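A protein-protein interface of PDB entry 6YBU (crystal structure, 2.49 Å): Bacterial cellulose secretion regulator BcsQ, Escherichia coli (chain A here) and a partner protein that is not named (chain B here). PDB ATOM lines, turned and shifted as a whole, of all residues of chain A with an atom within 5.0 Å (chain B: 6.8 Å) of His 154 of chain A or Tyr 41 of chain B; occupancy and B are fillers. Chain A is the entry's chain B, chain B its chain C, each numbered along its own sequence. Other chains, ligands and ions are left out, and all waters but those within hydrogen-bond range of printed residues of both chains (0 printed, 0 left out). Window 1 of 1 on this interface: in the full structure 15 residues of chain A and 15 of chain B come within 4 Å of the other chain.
The backbone carbonyl oxygen of Leu 186 of chain A sits at hydrogen-bond distance from the side-chain hydroxyl of Ser 190 of chain A. The backbone NH (N) of Ala 42 of chain B lies close to the side-chain carboxylate (OD1) of Asp 40 of chain B (3.4 Å). The indole nitrogen (NE1) of Trp 187 of chain A is in hydrogen-bond range of a ring nitrogen (ND1) of His 154 of chain A, 3.0 Å away. The backbone carbonyl oxygen (O) of His 154 of chain A sits at hydrogen-bond distance from a ring nitrogen (ND1) of His 158 of chain A, at 2.7 Å.
Of the 13 printed residues of chain A, 7 touch a printed residue of chain B. Printed residues of chain A that touch a printed residue of chain B: Ala 151, His 154, Ile 155, Leu 157, His 158, Leu 186 and Ser 190.
His 154 of chain A touches just these residues of chain B: Tyr 41 (3.8 Å), Leu 60 (3.4 Å) and Phe 63 (3.8 Å). Of the printed residues of chain B, Ile 155 of chain A touches Leu 59 (3.9 Å) and Phe 63 (3.96 Å). Of the printed residues of chain B, Leu 157 of chain A touches Ile 39. Printed residues of chain A within 4 Å of Tyr 41 of chain B: His 154 (3.8 Å), His 158 (2.4 Å) and Ser 190 (3.7 Å). Ala 64 of chain B touches none of the printed residues of chain A. The nearest residue of chain B that does not touch His 154 of chain A is Leu 59 of chain B (4.5 Å). The nearest printed residue of chain A that does not touch Tyr 41 of chain B is Leu 186 of chain A (4.004 Å). The nearest printed residue of chain A that does not touch Phe 63 of chain B is Arg 156 of chain A (6.2 Å).
CD2 of Leu 59 of chain B touches CB of Ala 151 of chain A (3.6 Å). Tyr 41 of chain B touches His 154 of chain A (OH to CE1, 3.8 Å). CG1 of Ile 155 of chain A touches CD1 of Leu 59 of chain B, at 3.9 Å. Phe 63 of chain B touches Ile 155 of chain A. Ile 39 of chain B touches Leu 157 of chain A (CD1 to O, 3.4 Å). NE2 of His 158 of chain A touches CD1 of Ile 39 of chain B, 3.6 Å away. His 158 of chain A touches Phe 63 of chain B (CG to CD1, 3.5 Å). Leu 60 of chain B touches Leu 186 of chain A. Ser 190 of chain A touches Ile 39 of chain B. Ser 190 of chain A touches Tyr 41 of chain B.
The backbone carbonyl oxygen (O) of Ser 190 of chain A lies within hydrogen-bond range of the backbone NH (N) of Asp 40 of chain B (2.9 Å). NE2 of His 158 of chain A sits at hydrogen-bond distance from OH of Tyr 41 of chain B (2.4 Å).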
ATOM      1  N   ASP A 150     -21.953 -30.649  12.436  1.00  0.00           N
ATOM      2  CA  ASP A 150     -22.895 -29.585  12.126  1.00  0.00           C
ATOM      3  C   ASP A 150     -22.128 -28.421  11.514  1.00  0.00           C
ATOM      4  O   ASP A 150     -20.895 -28.420  11.458  1.00  0.00           O
ATOM      5  CB  ASP A 150     -23.691 -29.147  13.363  1.00  0.00           C
ATOM      6  CG  ASP A 150     -22.804 -28.792  14.542  1.00  0.00           C
ATOM      7  OD1 ASP A 150     -21.914 -27.930  14.385  1.00  0.00           O
ATOM      8  OD2 ASP A 150     -23.010 -29.367  15.632  1.00  0.00           O
ATOM      9  N   ALA A 151     -22.882 -27.419  11.053  1.00  0.00           N
ATOM     10  CA  ALA A 151     -22.275 -26.281  10.371  1.00  0.00           C
ATOM     11  C   ALA A 151     -21.403 -25.451  11.307  1.00  0.00           C
ATOM     12  O   ALA A 151     -20.420 -24.848  10.859  1.00  0.00           O
ATOM     13  CB  ALA A 151     -23.362 -25.410   9.747  1.00  0.00           C
ATOM     14  N   ASN A 152     -21.746 -25.402  12.596  1.00  0.00           N
ATOM     15  CA  ASN A 152     -20.948 -24.648  13.558  1.00  0.00           C
ATOM     16  C   ASN A 152     -19.521 -25.181  13.619  1.00  0.00           C
ATOM     17  O   ASN A 152     -18.554 -24.436  13.425  1.00  0.00           O
ATOM     18  CB  ASN A 152     -21.615 -24.703  14.937  1.00  0.00           C
ATOM     19  CG  ASN A 152     -20.870 -23.897  15.994  1.00  0.00           C
ATOM     20  OD1 ASN A 152     -19.687 -24.120  16.253  1.00  0.00           O
ATOM     21  ND2 ASN A 152     -21.572 -22.957  16.616  1.00  0.00           N
ATOM     22  N   CYS A 153     -19.372 -26.479  13.894  1.00  0.00           N
ATOM     23  CA  CYS A 153     -18.041 -27.072  13.964  1.00  0.00           C
ATOM     24  C   CYS A 153     -17.328 -27.018  12.621  1.00  0.00           C
ATOM     25  O   CYS A 153     -16.099 -26.893  12.578  1.00  0.00           O
ATOM     26  CB  CYS A 153     -18.133 -28.516  14.456  1.00  0.00           C
ATOM     27  SG  CYS A 153     -18.695 -28.691  16.168  1.00  0.00           S
ATOM     28  N   HIS A 154     -18.075 -27.120  11.520  1.00  0.00           N
ATOM     29  CA  HIS A 154     -17.465 -27.009  10.198  1.00  0.00           C
ATOM     30  C   HIS A 154     -16.796 -25.651  10.020  1.00  0.00           C
ATOM     31  O   HIS A 154     -15.666 -25.562   9.526  1.00  0.00           O
ATOM     32  CB  HIS A 154     -18.521 -27.234   9.113  1.00  0.00           C
ATOM     33  CG  HIS A 154     -17.983 -27.128   7.720  1.00  0.00           C
ATOM     34  ND1 HIS A 154     -17.210 -28.112   7.144  1.00  0.00           N
ATOM     35  CD2 HIS A 154     -18.103 -26.152   6.789  1.00  0.00           C
ATOM     36  CE1 HIS A 154     -16.880 -27.749   5.917  1.00  0.00           C
ATOM     37  NE2 HIS A 154     -17.408 -26.562   5.678  1.00  0.00           N
ATOM     38  N   ILE A 155     -17.486 -24.580  10.418  1.00  0.00           N
ATOM     39  CA  ILE A 155     -16.893 -23.247  10.361  1.00  0.00           C
ATOM     40  C   ILE A 155     -15.670 -23.170  11.266  1.00  0.00           C
ATOM     41  O   ILE A 155     -14.626 -22.629  10.881  1.00  0.00           O
ATOM     42  CB  ILE A 155     -17.939 -22.182  10.737  1.00  0.00           C
ATOM     43  CG1 ILE A 155     -19.090 -22.171   9.730  1.00  0.00           C
ATOM     44  CG2 ILE A 155     -17.290 -20.811  10.814  1.00  0.00           C
ATOM     45  CD1 ILE A 155     -20.343 -21.494  10.248  1.00  0.00           C
ATOM     46  N   ARG A 156     -15.780 -23.720  12.480  1.00  0.00           N
ATOM     47  CA  ARG A 156     -14.696 -23.612  13.453  1.00  0.00           C
ATOM     48  C   ARG A 156     -13.433 -24.311  12.965  1.00  0.00           C
ATOM     49  O   ARG A 156     -12.319 -23.837  13.218  1.00  0.00           O
ATOM     50  CB  ARG A 156     -15.140 -24.189  14.796  1.00  0.00           C
ATOM     51  CG  ARG A 156     -16.236 -23.389  15.480  1.00  0.00           C
ATOM     52  CD  ARG A 156     -16.536 -23.962  16.854  1.00  0.00           C
ATOM     53  NE  ARG A 156     -17.474 -23.138  17.608  1.00  0.00           N
ATOM     54  CZ  ARG A 156     -17.120 -22.091  18.346  1.00  0.00           C
ATOM     55  NH1 ARG A 156     -15.844 -21.735  18.424  1.00  0.00           N
ATOM     56  NH2 ARG A 156     -18.040 -21.398  19.000  1.00  0.00           N
ATOM     57  N   LEU A 157     -13.581 -25.435  12.262  1.00  0.00           N
ATOM     58  CA  LEU A 157     -12.418 -26.133  11.728  1.00  0.00           C
ATOM     59  C   LEU A 157     -11.685 -25.325  10.665  1.00  0.00           C
ATOM     60  O   LEU A 157     -10.559 -25.688  10.305  1.00  0.00           O
ATOM     61  CB  LEU A 157     -12.833 -27.488  11.150  1.00  0.00           C
ATOM     62  CG  LEU A 157     -13.319 -28.556  12.136  1.00  0.00           C
ATOM     63  CD1 LEU A 157     -13.719 -29.822  11.395  1.00  0.00           C
ATOM     64  CD2 LEU A 157     -12.248 -28.861  13.175  1.00  0.00           C
ATOM     65  N   HIS A 158     -12.288 -24.246  10.161  1.00  0.00           N
ATOM     66  CA  HIS A 158     -11.656 -23.384   9.174  1.00  0.00           C
ATOM     67  C   HIS A 158     -11.197 -22.044   9.734  1.00  0.00           C
ATOM     68  O   HIS A 158     -10.429 -21.348   9.060  1.00  0.00           O
ATOM     69  CB  HIS A 158     -12.611 -23.120   7.999  1.00  0.00           C
ATOM     70  CG  HIS A 158     -12.939 -24.339   7.194  1.00  0.00           C
ATOM     71  ND1 HIS A 158     -13.753 -25.347   7.666  1.00  0.00           N
ATOM     72  CD2 HIS A 158     -12.569 -24.709   5.945  1.00  0.00           C
ATOM     73  CE1 HIS A 158     -13.867 -26.286   6.744  1.00  0.00           C
ATOM     74  NE2 HIS A 158     -13.158 -25.923   5.690  1.00  0.00           N
ATOM     75  N   ILE A 183     -22.147 -32.858   5.298  1.00  0.00           N
ATOM     76  CA  ILE A 183     -20.949 -32.373   5.979  1.00  0.00           C
ATOM     77  C   ILE A 183     -19.986 -33.523   6.242  1.00  0.00           C
ATOM     78  O   ILE A 183     -18.762 -33.366   6.142  1.00  0.00           O
ATOM     79  CB  ILE A 183     -21.333 -31.648   7.284  1.00  0.00           C
ATOM     80  CG1 ILE A 183     -22.206 -30.426   6.989  1.00  0.00           C
ATOM     81  CG2 ILE A 183     -20.088 -31.241   8.064  1.00  0.00           C
ATOM     82  CD1 ILE A 183     -22.762 -29.758   8.234  1.00  0.00           C
ATOM     83  N   LEU A 186     -18.190 -34.661   3.060  1.00  0.00           N
ATOM     84  CA  LEU A 186     -17.180 -33.663   2.730  1.00  0.00           C
ATOM     85  C   LEU A 186     -15.971 -33.775   3.653  1.00  0.00           C
ATOM     86  O   LEU A 186     -14.826 -33.670   3.199  1.00  0.00           O
ATOM     87  CB  LEU A 186     -17.791 -32.263   2.801  1.00  0.00           C
ATOM     88  CG  LEU A 186     -16.875 -31.090   2.450  1.00  0.00           C
ATOM     89  CD1 LEU A 186     -16.256 -31.288   1.077  1.00  0.00           C
ATOM     90  CD2 LEU A 186     -17.646 -29.782   2.506  1.00  0.00           C
ATOM     91  N   TRP A 187     -16.207 -33.996   4.949  1.00  0.00           N
ATOM     92  CA  TRP A 187     -15.101 -34.153   5.890  1.00  0.00           C
ATOM     93  C   TRP A 187     -14.241 -35.361   5.539  1.00  0.00           C
ATOM     94  O   TRP A 187     -13.014 -35.320   5.683  1.00  0.00           O
ATOM     95  CB  TRP A 187     -15.636 -34.283   7.316  1.00  0.00           C
ATOM     96  CG  TRP A 187     -16.074 -32.992   7.932  1.00  0.00           C
ATOM     97  CD1 TRP A 187     -16.142 -31.774   7.324  1.00  0.00           C
ATOM     98  CD2 TRP A 187     -16.502 -32.792   9.284  1.00  0.00           C
ATOM     99  NE1 TRP A 187     -16.589 -30.826   8.214  1.00  0.00           N
ATOM    100  CE2 TRP A 187     -16.815 -31.426   9.426  1.00  0.00           C
ATOM    101  CE3 TRP A 187     -16.651 -33.637  10.391  1.00  0.00           C
ATOM    102  CZ2 TRP A 187     -17.268 -30.883  10.628  1.00  0.00           C
ATOM    103  CZ3 TRP A 187     -17.100 -33.096  11.583  1.00  0.00           C
ATOM    104  CH2 TRP A 187     -17.403 -31.732  11.692  1.00  0.00           C
ATOM    105  N   SER A 190     -11.915 -34.136   2.873  1.00  0.00           N
ATOM    106  CA  SER A 190     -11.169 -32.904   3.105  1.00  0.00           C
ATOM    107  C   SER A 190     -10.447 -32.853   4.443  1.00  0.00           C
ATOM    108  O   SER A 190      -9.358 -32.277   4.511  1.00  0.00           O
ATOM    109  CB  SER A 190     -12.102 -31.685   3.005  1.00  0.00           C
ATOM    110  OG  SER A 190     -13.058 -31.675   4.049  1.00  0.00           O
ATOM    111  N   ILE B  39      -6.660 -29.181   6.109  1.00  0.00           N
ATOM    112  CA  ILE B  39      -7.825 -29.435   5.272  1.00  0.00           C
ATOM    113  C   ILE B  39      -7.367 -29.388   3.822  1.00  0.00           C
ATOM    114  O   ILE B  39      -6.661 -28.455   3.421  1.00  0.00           O
ATOM    115  CB  ILE B  39      -8.948 -28.414   5.529  1.00  0.00           C
ATOM    116  CG1 ILE B  39      -9.273 -28.329   7.024  1.00  0.00           C
ATOM    117  CG2 ILE B  39     -10.188 -28.789   4.741  1.00  0.00           C
ATOM    118  CD1 ILE B  39     -10.329 -27.303   7.369  1.00  0.00           C
ATOM    119  N   ASP B  40      -7.762 -30.393   3.041  1.00  0.00           N
ATOM    120  CA  ASP B  40      -7.293 -30.552   1.666  1.00  0.00           C
ATOM    121  C   ASP B  40      -8.495 -30.742   0.744  1.00  0.00           C
ATOM    122  O   ASP B  40      -9.008 -31.858   0.601  1.00  0.00           O
ATOM    123  CB  ASP B  40      -6.322 -31.726   1.556  1.00  0.00           C
ATOM    124  CG  ASP B  40      -5.971 -32.059   0.121  1.00  0.00           C
ATOM    125  OD1 ASP B  40      -5.646 -31.127  -0.644  1.00  0.00           O
ATOM    126  OD2 ASP B  40      -6.015 -33.255  -0.240  1.00  0.00           O
ATOM    127  N   TYR B  41      -8.941 -29.652   0.122  1.00  0.00           N
ATOM    128  CA  TYR B  41      -9.988 -29.690  -0.900  1.00  0.00           C
ATOM    129  C   TYR B  41      -9.429 -29.982  -2.283  1.00  0.00           C
ATOM    130  O   TYR B  41      -9.822 -29.332  -3.256  1.00  0.00           O
ATOM    131  CB  TYR B  41     -10.760 -28.374  -0.906  1.00  0.00           C
ATOM    132  CG  TYR B  41     -11.559 -28.083   0.346  1.00  0.00           C
ATOM    133  CD1 TYR B  41     -12.751 -28.747   0.606  1.00  0.00           C
ATOM    134  CD2 TYR B  41     -11.132 -27.125   1.256  1.00  0.00           C
ATOM    135  CE1 TYR B  41     -13.487 -28.475   1.748  1.00  0.00           C
ATOM    136  CE2 TYR B  41     -11.863 -26.847   2.396  1.00  0.00           C
ATOM    137  CZ  TYR B  41     -13.036 -27.524   2.638  1.00  0.00           C
ATOM    138  OH  TYR B  41     -13.758 -27.243   3.774  1.00  0.00           O
ATOM    139  N   ALA B  42      -8.515 -30.948  -2.400  1.00  0.00           N
ATOM    140  CA  ALA B  42      -7.807 -31.171  -3.659  1.00  0.00           C
ATOM    141  C   ALA B  42      -8.776 -31.459  -4.801  1.00  0.00           C
ATOM    142  O   ALA B  42      -8.874 -30.684  -5.760  1.00  0.00           O
ATOM    143  CB  ALA B  42      -6.804 -32.316  -3.499  1.00  0.00           C
ATOM    144  N   ASP B  43      -9.506 -32.570  -4.713  1.00  0.00           N
ATOM    145  CA  ASP B  43     -10.431 -32.990  -5.764  1.00  0.00           C
ATOM    146  C   ASP B  43     -11.812 -33.255  -5.162  1.00  0.00           C
ATOM    147  O   ASP B  43     -12.335 -34.369  -5.205  1.00  0.00           O
ATOM    148  CB  ASP B  43      -9.913 -34.228  -6.493  1.00  0.00           C
ATOM    149  CG  ASP B  43      -8.603 -33.978  -7.213  1.00  0.00           C
ATOM    150  OD1 ASP B  43      -8.319 -32.811  -7.553  1.00  0.00           O
ATOM    151  OD2 ASP B  43      -7.858 -34.952  -7.447  1.00  0.00           O
ATOM    152  N   ILE B  44     -12.414 -32.209  -4.591  1.00  0.00           N
ATOM    153  CA  ILE B  44     -13.767 -32.343  -4.060  1.00  0.00           C
ATOM    154  C   ILE B  44     -14.786 -32.398  -5.190  1.00  0.00           C
ATOM    155  O   ILE B  44     -15.839 -33.036  -5.058  1.00  0.00           O
ATOM    156  CB  ILE B  44     -14.073 -31.197  -3.080  1.00  0.00           C
ATOM    157  CG1 ILE B  44     -13.016 -31.141  -1.982  1.00  0.00           C
ATOM    158  CG2 ILE B  44     -15.442 -31.386  -2.455  1.00  0.00           C
ATOM    159  CD1 ILE B  44     -13.054 -32.330  -1.049  1.00  0.00           C
ATOM    160  N   SER B  45     -14.488 -31.753  -6.320  1.00  0.00           N
ATOM    161  CA  SER B  45     -15.449 -31.683  -7.416  1.00  0.00           C
ATOM    162  C   SER B  45     -15.727 -33.053  -8.023  1.00  0.00           C
ATOM    163  O   SER B  45     -16.799 -33.264  -8.602  1.00  0.00           O
ATOM    164  CB  SER B  45     -14.939 -30.724  -8.493  1.00  0.00           C
ATOM    165  OG  SER B  45     -15.669 -30.870  -9.700  1.00  0.00           O
ATOM    166  N   LEU B  54     -22.103 -29.300  -2.372  1.00  0.00           N
ATOM    167  CA  LEU B  54     -21.500 -27.981  -2.536  1.00  0.00           C
ATOM    168  C   LEU B  54     -22.416 -27.034  -3.302  1.00  0.00           C
ATOM    169  O   LEU B  54     -22.338 -25.815  -3.116  1.00  0.00           O
ATOM    170  CB  LEU B  54     -20.153 -28.100  -3.247  1.00  0.00           C
ATOM    171  CG  LEU B  54     -19.019 -28.782  -2.483  1.00  0.00           C
ATOM    172  CD1 LEU B  54     -17.806 -28.880  -3.382  1.00  0.00           C
ATOM    173  CD2 LEU B  54     -18.686 -28.029  -1.205  1.00  0.00           C
ATOM    174  N   LEU B  59     -22.519 -22.597   2.389  1.00  0.00           N
ATOM    175  CA  LEU B  59     -21.477 -22.566   3.409  1.00  0.00           C
ATOM    176  C   LEU B  59     -20.351 -23.542   3.083  1.00  0.00           C
ATOM    177  O   LEU B  59     -19.169 -23.203   3.216  1.00  0.00           O
ATOM    178  CB  LEU B  59     -22.080 -22.880   4.775  1.00  0.00           C
ATOM    179  CG  LEU B  59     -21.123 -22.825   5.964  1.00  0.00           C
ATOM    180  CD1 LEU B  59     -20.777 -21.388   6.322  1.00  0.00           C
ATOM    181  CD2 LEU B  59     -21.712 -23.557   7.154  1.00  0.00           C
ATOM    182  N   LEU B  60     -20.699 -24.758   2.656  1.00  0.00           N
ATOM    183  CA  LEU B  60     -19.676 -25.733   2.290  1.00  0.00           C
ATOM    184  C   LEU B  60     -18.930 -25.301   1.035  1.00  0.00           C
ATOM    185  O   LEU B  60     -17.702 -25.428   0.964  1.00  0.00           O
ATOM    186  CB  LEU B  60     -20.310 -27.110   2.094  1.00  0.00           C
ATOM    187  CG  LEU B  60     -21.230 -27.592   3.217  1.00  0.00           C
ATOM    188  CD1 LEU B  60     -21.731 -29.002   2.941  1.00  0.00           C
ATOM    189  CD2 LEU B  60     -20.519 -27.526   4.563  1.00  0.00           C
ATOM    190  N   ALA B  61     -19.654 -24.789   0.035  1.00  0.00           N
ATOM    191  CA  ALA B  61     -19.004 -24.298  -1.176  1.00  0.00           C
ATOM    192  C   ALA B  61     -18.086 -23.119  -0.881  1.00  0.00           C
ATOM    193  O   ALA B  61     -17.053 -22.956  -1.541  1.00  0.00           O
ATOM    194  CB  ALA B  61     -20.053 -23.897  -2.213  1.00  0.00           C
ATOM    195  N   PHE B  63     -16.162 -22.517   1.762  1.00  0.00           N
ATOM    196  CA  PHE B  63     -14.872 -22.960   2.273  1.00  0.00           C
ATOM    197  C   PHE B  63     -14.120 -23.851   1.295  1.00  0.00           C
ATOM    198  O   PHE B  63     -12.895 -23.971   1.405  1.00  0.00           O
ATOM    199  CB  PHE B  63     -15.052 -23.696   3.602  1.00  0.00           C
ATOM    200  CG  PHE B  63     -15.485 -22.809   4.728  1.00  0.00           C
ATOM    201  CD1 PHE B  63     -14.602 -21.902   5.285  1.00  0.00           C
ATOM    202  CD2 PHE B  63     -16.770 -22.882   5.234  1.00  0.00           C
ATOM    203  CE1 PHE B  63     -14.993 -21.081   6.323  1.00  0.00           C
ATOM    204  CE2 PHE B  63     -17.166 -22.065   6.274  1.00  0.00           C
ATOM    205  CZ  PHE B  63     -16.276 -21.164   6.819  1.00  0.00           C
ATOM    206  N   ALA B  64     -14.814 -24.475   0.347  1.00  0.00           N
ATOM    207  CA  ALA B  64     -14.159 -25.297  -0.662  1.00  0.00           C
ATOM    208  C   ALA B  64     -13.419 -24.473  -1.708  1.00  0.00           C
ATOM    209  O   ALA B  64     -12.783 -25.056  -2.594  1.00  0.00           O
ATOM    210  CB  ALA B  64     -15.182 -26.205  -1.350  1.00  0.00           C
ATOM    211  N   GLN B  65     -13.490 -23.148  -1.634  1.00  0.00           N
ATOM    212  CA  GLN B  65     -12.764 -22.286  -2.560  1.00  0.00           C
ATOM    213  C   GLN B  65     -12.396 -20.961  -1.897  1.00  0.00           C
ATOM    214  O   GLN B  65     -11.445 -20.892  -1.117  1.00  0.00           O
ATOM    215  CB  GLN B  65     -13.589 -22.040  -3.824  1.00  0.00           C
ATOM    216  CG  GLN B  65     -12.867 -21.226  -4.891  1.00  0.00           C
ATOM    217  CD  GLN B  65     -11.667 -21.950  -5.483  1.00  0.00           C
ATOM    218  OE1 GLN B  65     -11.449 -23.137  -5.229  1.00  0.00           O
ATOM    219  NE2 GLN B  65     -10.882 -21.237  -6.284  1.00  0.00           N
